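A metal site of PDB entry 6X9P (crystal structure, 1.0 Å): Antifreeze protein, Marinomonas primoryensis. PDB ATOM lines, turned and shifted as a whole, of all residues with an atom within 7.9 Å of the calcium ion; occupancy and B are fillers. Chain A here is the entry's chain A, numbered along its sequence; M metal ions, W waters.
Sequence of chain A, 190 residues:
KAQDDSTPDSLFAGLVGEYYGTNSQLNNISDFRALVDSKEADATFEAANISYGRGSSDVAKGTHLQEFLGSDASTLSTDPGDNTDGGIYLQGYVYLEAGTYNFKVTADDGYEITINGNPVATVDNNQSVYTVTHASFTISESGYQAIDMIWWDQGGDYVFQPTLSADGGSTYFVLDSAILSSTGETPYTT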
ATOM      1  N   THR A  22     -10.542  19.487 -24.993  1.00  0.00           N
ATOM      2  CA  THR A  22     -11.566  18.469 -24.735  1.00  0.00           C
ATOM      3  C   THR A  22     -12.300  18.809 -23.448  1.00  0.00           C
ATOM      4  O   THR A  22     -11.776  19.520 -22.587  1.00  0.00           O
ATOM      5  CB  THR A  22     -10.932  17.070 -24.660  1.00  0.00           C
ATOM      6  OG1 THR A  22     -11.943  16.071 -24.500  1.00  0.00           O
ATOM      7  CG2 THR A  22      -9.981  16.902 -23.491  1.00  0.00           C
ATOM      8  N   ASN A  23     -13.511  18.268 -23.315  1.00  0.00           N
ATOM      9  CA  ASN A  23     -14.278  18.358 -22.077  1.00  0.00           C
ATOM     10  C   ASN A  23     -14.296  17.037 -21.318  1.00  0.00           C
ATOM     11  O   ASN A  23     -15.020  16.896 -20.327  1.00  0.00           O
ATOM     12  CB  ASN A  23     -15.680  18.888 -22.343  1.00  0.00           C
ATOM     13  CG  ASN A  23     -15.629  20.247 -23.014  1.00  0.00           C
ATOM     14  OD1 ASN A  23     -14.825  21.109 -22.619  1.00  0.00           O
ATOM     15  ND2 ASN A  23     -16.450  20.426 -24.028  1.00  0.00           N
ATOM     16  N   SER A  24     -13.465  16.092 -21.745  1.00  0.00           N
ATOM     17  CA  SER A  24     -13.155  14.886 -20.990  1.00  0.00           C
ATOM     18  C   SER A  24     -11.877  15.102 -20.180  1.00  0.00           C
ATOM     19  O   SER A  24     -11.103  16.035 -20.430  1.00  0.00           O
ATOM     20  CB  SER A  24     -12.978  13.724 -21.952  1.00  0.00           C
ATOM     21  OG  SER A  24     -11.790  13.829 -22.730  1.00  0.00           O
ATOM     22  N   GLN A  25     -11.666  14.226 -19.205  1.00  0.00           N
ATOM     23  CA  GLN A  25     -10.509  14.344 -18.332  1.00  0.00           C
ATOM     24  C   GLN A  25      -9.262  13.762 -18.997  1.00  0.00           C
ATOM     25  O   GLN A  25      -9.264  12.618 -19.469  1.00  0.00           O
ATOM     26  CB  GLN A  25     -10.780  13.615 -17.008  1.00  0.00           C
ATOM     27  CG  GLN A  25      -9.549  13.394 -16.128  1.00  0.00           C
ATOM     28  CD  GLN A  25      -8.963  14.675 -15.534  1.00  0.00           C
ATOM     29  OE1 GLN A  25      -9.316  15.789 -15.895  1.00  0.00           O
ATOM     30  NE2 GLN A  25      -8.022  14.496 -14.621  1.00  0.00           N
ATOM     31  N   LEU A  26      -8.169  14.504 -18.933  1.00  0.00           N
ATOM     32  CA  LEU A  26      -6.851  14.015 -19.310  1.00  0.00           C
ATOM     33  C   LEU A  26      -6.085  13.604 -18.062  1.00  0.00           C
ATOM     34  O   LEU A  26      -5.728  14.461 -17.246  1.00  0.00           O
ATOM     35  CB  LEU A  26      -6.094  15.087 -20.080  1.00  0.00           C
ATOM     36  CG  LEU A  26      -6.760  15.545 -21.389  1.00  0.00           C
ATOM     37  CD1 LEU A  26      -5.963  16.730 -21.971  1.00  0.00           C
ATOM     38  CD2 LEU A  26      -6.840  14.421 -22.388  1.00  0.00           C
ATOM     39  N   ASN A  27      -5.839  12.304 -17.891  1.00  0.00           N
ATOM     40  CA  ASN A  27      -5.134  11.788 -16.721  1.00  0.00           C
ATOM     41  C   ASN A  27      -3.689  11.378 -16.991  1.00  0.00           C
ATOM     42  O   ASN A  27      -2.919  11.207 -16.046  1.00  0.00           O
ATOM     43  CB  ASN A  27      -5.831  10.534 -16.155  1.00  0.00           C
ATOM     44  CG  ASN A  27      -7.041  10.875 -15.338  1.00  0.00           C
ATOM     45  OD1 ASN A  27      -6.999  11.775 -14.495  1.00  0.00           O
ATOM     46  ND2 ASN A  27      -8.138  10.194 -15.611  1.00  0.00           N
ATOM     47  N   ASP A  58      -7.098  27.231 -15.989  1.00  0.00           N
ATOM     48  CA  ASP A  58      -7.293  26.260 -17.078  1.00  0.00           C
ATOM     49  C   ASP A  58      -6.723  26.746 -18.412  1.00  0.00           C
ATOM     50  O   ASP A  58      -7.161  27.771 -18.950  1.00  0.00           O
ATOM     51  CB  ASP A  58      -8.780  25.902 -17.298  1.00  0.00           C
ATOM     52  CG  ASP A  58      -9.527  25.524 -16.046  1.00  0.00           C
ATOM     53  OD1 ASP A  58      -8.984  24.822 -15.207  1.00  0.00           O
ATOM     54  OD2 ASP A  58     -10.707  25.879 -15.962  1.00  0.00           O
ATOM     55  N   THR A  84     -12.488  22.239 -21.029  1.00  0.00           N
ATOM     56  CA  THR A  84     -12.001  22.106 -19.657  1.00  0.00           C
ATOM     57  C   THR A  84     -10.538  21.703 -19.617  1.00  0.00           C
ATOM     58  O   THR A  84      -9.811  22.115 -18.693  1.00  0.00           O
ATOM     59  CB  THR A  84     -12.853  21.090 -18.867  1.00  0.00           C
ATOM     60  OG1 THR A  84     -12.723  19.775 -19.409  1.00  0.00           O
ATOM     61  CG2 THR A  84     -14.322  21.447 -18.877  1.00  0.00           C
ATOM     62  N   ASP A  85     -10.095  20.882 -20.569  1.00  0.00           N
ATOM     63  CA  ASP A  85      -8.791  20.272 -20.601  1.00  0.00           C
ATOM     64  C   ASP A  85      -8.170  20.513 -21.971  1.00  0.00           C
ATOM     65  O   ASP A  85      -8.907  20.677 -22.964  1.00  0.00           O
ATOM     66  CB  ASP A  85      -8.904  18.730 -20.382  1.00  0.00           C
ATOM     67  CG  ASP A  85      -9.366  18.328 -18.982  1.00  0.00           C
ATOM     68  OD1 ASP A  85     -10.399  18.868 -18.487  1.00  0.00           O
ATOM     69  OD2 ASP A  85      -8.717  17.443 -18.368  1.00  0.00           O
ATOM     70  N   GLY A  86      -6.847  20.528 -22.064  1.00  0.00           N
ATOM     71  CA  GLY A  86      -6.251  20.693 -23.388  1.00  0.00           C
ATOM     72  C   GLY A  86      -4.761  20.468 -23.347  1.00  0.00           C
ATOM     73  O   GLY A  86      -4.160  20.373 -22.286  1.00  0.00           O
ATOM     74  N   ASP A 109       0.530  19.992 -16.583  1.00  0.00           N
ATOM     75  CA  ASP A 109       0.545  18.663 -15.949  1.00  0.00           C
ATOM     76  C   ASP A 109       1.700  17.838 -16.522  1.00  0.00           C
ATOM     77  O   ASP A 109       2.856  18.209 -16.305  1.00  0.00           O
ATOM     78  CB  ASP A 109      -0.859  18.040 -16.083  1.00  0.00           C
ATOM     79  CG  ASP A 109      -1.822  18.661 -15.098  1.00  0.00           C
ATOM     80  OD1 ASP A 109      -1.756  18.250 -13.925  1.00  0.00           O
ATOM     81  OD2 ASP A 109      -2.601  19.575 -15.490  1.00  0.00           O
ATOM     82  N   ASN A 126      -0.832  13.550 -13.958  1.00  0.00           N
ATOM     83  CA  ASN A 126      -1.075  14.939 -13.607  1.00  0.00           C
ATOM     84  C   ASN A 126      -0.201  15.336 -12.434  1.00  0.00           C
ATOM     85  O   ASN A 126       0.225  14.497 -11.627  1.00  0.00           O
ATOM     86  CB  ASN A 126      -2.553  15.142 -13.304  1.00  0.00           C
ATOM     87  CG  ASN A 126      -3.378  15.070 -14.559  1.00  0.00           C
ATOM     88  OD1 ASN A 126      -2.916  15.469 -15.619  1.00  0.00           O
ATOM     89  ND2 ASN A 126      -4.605  14.578 -14.452  1.00  0.00           N
ATOM     90  N   TRP A 152       0.086  18.380 -21.569  1.00  0.00           N
ATOM     91  CA  TRP A 152      -1.320  18.735 -21.383  1.00  0.00           C
ATOM     92  C   TRP A 152      -1.544  19.358 -20.028  1.00  0.00           C
ATOM     93  O   TRP A 152      -0.715  19.264 -19.113  1.00  0.00           O
ATOM     94  CB  TRP A 152      -2.263  17.502 -21.594  1.00  0.00           C
ATOM     95  CG  TRP A 152      -2.221  16.570 -20.409  1.00  0.00           C
ATOM     96  CD1 TRP A 152      -3.053  16.603 -19.310  1.00  0.00           C
ATOM     97  CD2 TRP A 152      -1.278  15.534 -20.157  1.00  0.00           C
ATOM     98  NE1 TRP A 152      -2.678  15.647 -18.393  1.00  0.00           N
ATOM     99  CE2 TRP A 152      -1.589  14.989 -18.875  1.00  0.00           C
ATOM    100  CE3 TRP A 152      -0.204  15.012 -20.864  1.00  0.00           C
ATOM    101  CZ2 TRP A 152      -0.837  13.961 -18.313  1.00  0.00           C
ATOM    102  CZ3 TRP A 152       0.541  13.994 -20.294  1.00  0.00           C
ATOM    103  CH2 TRP A 152       0.212  13.476 -19.030  1.00  0.00           C
ATOM    104  N   ASP A 153      -2.733  19.968 -19.910  1.00  0.00           N
ATOM    105  CA  ASP A 153      -3.298  20.506 -18.680  1.00  0.00           C
ATOM    106  C   ASP A 153      -4.655  19.845 -18.459  1.00  0.00           C
ATOM    107  O   ASP A 153      -5.554  19.921 -19.320  1.00  0.00           O
ATOM    108  CB  ASP A 153      -3.505  22.027 -18.803  1.00  0.00           C
ATOM    109  CG  ASP A 153      -4.193  22.630 -17.596  1.00  0.00           C
ATOM    110  OD1 ASP A 153      -3.880  22.141 -16.475  1.00  0.00           O
ATOM    111  OD2 ASP A 153      -5.043  23.533 -17.771  1.00  0.00           O
ATOM    112  N   GLN A 154      -4.826  19.216 -17.294  1.00  0.00           N
ATOM    113  CA  GLN A 154      -6.122  18.664 -16.888  1.00  0.00           C
ATOM    114  C   GLN A 154      -7.022  19.718 -16.260  1.00  0.00           C
ATOM    115  O   GLN A 154      -8.180  19.428 -15.929  1.00  0.00           O
ATOM    116  CB  GLN A 154      -5.926  17.494 -15.905  1.00  0.00           C
ATOM    117  CG  GLN A 154      -5.377  17.905 -14.550  1.00  0.00           C
ATOM    118  CD  GLN A 154      -6.445  18.069 -13.507  1.00  0.00           C
ATOM    119  OE1 GLN A 154      -7.327  17.222 -13.345  1.00  0.00           O
ATOM    120  NE2 GLN A 154      -6.372  19.170 -12.760  1.00  0.00           N
ATOM    121  N   GLY A 155      -6.504  20.927 -16.062  1.00  0.00           N
ATOM    122  CA  GLY A 155      -7.210  21.993 -15.401  1.00  0.00           C
ATOM    123  C   GLY A 155      -6.330  22.645 -14.351  1.00  0.00           C
ATOM    124  O   GLY A 155      -5.331  22.076 -13.899  1.00  0.00           O
ATOM    125  N   GLY A 156      -6.727  23.841 -13.937  1.00  0.00           N
ATOM    126  CA  GLY A 156      -6.017  24.560 -12.888  1.00  0.00           C
ATOM    127  C   GLY A 156      -4.844  25.363 -13.454  1.00  0.00           C
ATOM    128  O   GLY A 156      -5.011  26.121 -14.403  1.00  0.00           O
HETATM  129 CA    CA M   1     -10.008  17.984 -16.268  1.00  0.00          CA
HETATM  130  O   HOH W   1      -9.774  17.929 -13.858  1.00  0.00           O
HETATM  131  O   HOH W   2     -11.381  19.806 -15.524  1.00  0.00           O
HETATM  132  O   HOH W   3     -12.074  16.829 -16.462  1.00  0.00           O
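The backbone carbonyl oxygen of Asp 85 sits at hydrogen-bond distance from the backbone NH of Thr 22 (2.9 Å).
The backbone NH (N) of Leu 26 sits close to the side-chain carboxylate (OD2) of Asp 85 (3.0 Å).
OD1 of Asn 27 is in hydrogen-bond range of NE2 of Gln 25, 2.9 Å away.
The side-chain amide nitrogen of Gln 25 sits close to the side-chain amide nitrogen of Asn 126 (3.4 Å).
The side-chain carboxylate (OD2) of Asp 109 sits close to the backbone NH (N) of Gln 154 (2.9 Å).
The side-chain carboxylate (OD1) of Asp 85 lies close to the side-chain hydroxyl (OG1) of Thr 84.
Three residues have an atom within 4 Å of the calcium ion: Gln 25, Asp 85 and Gln 154.
The calcium ion is bound by the side-chain amide oxygen (OE1) of Gln 25 (2.3 Å), the backbone carbonyl oxygen (O) of Gln 154 (2.4 Å), water W3 (2.4 Å), water W2 (2.4 Å), the side-chain carboxylate (OD1) of Asp 85 (2.4 Å), water W1 (2.4 Å) and the side-chain carboxylate (OD2) of Asp 85 (2.5 Å).
The calcium ion has seven donor atoms within binding distance.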
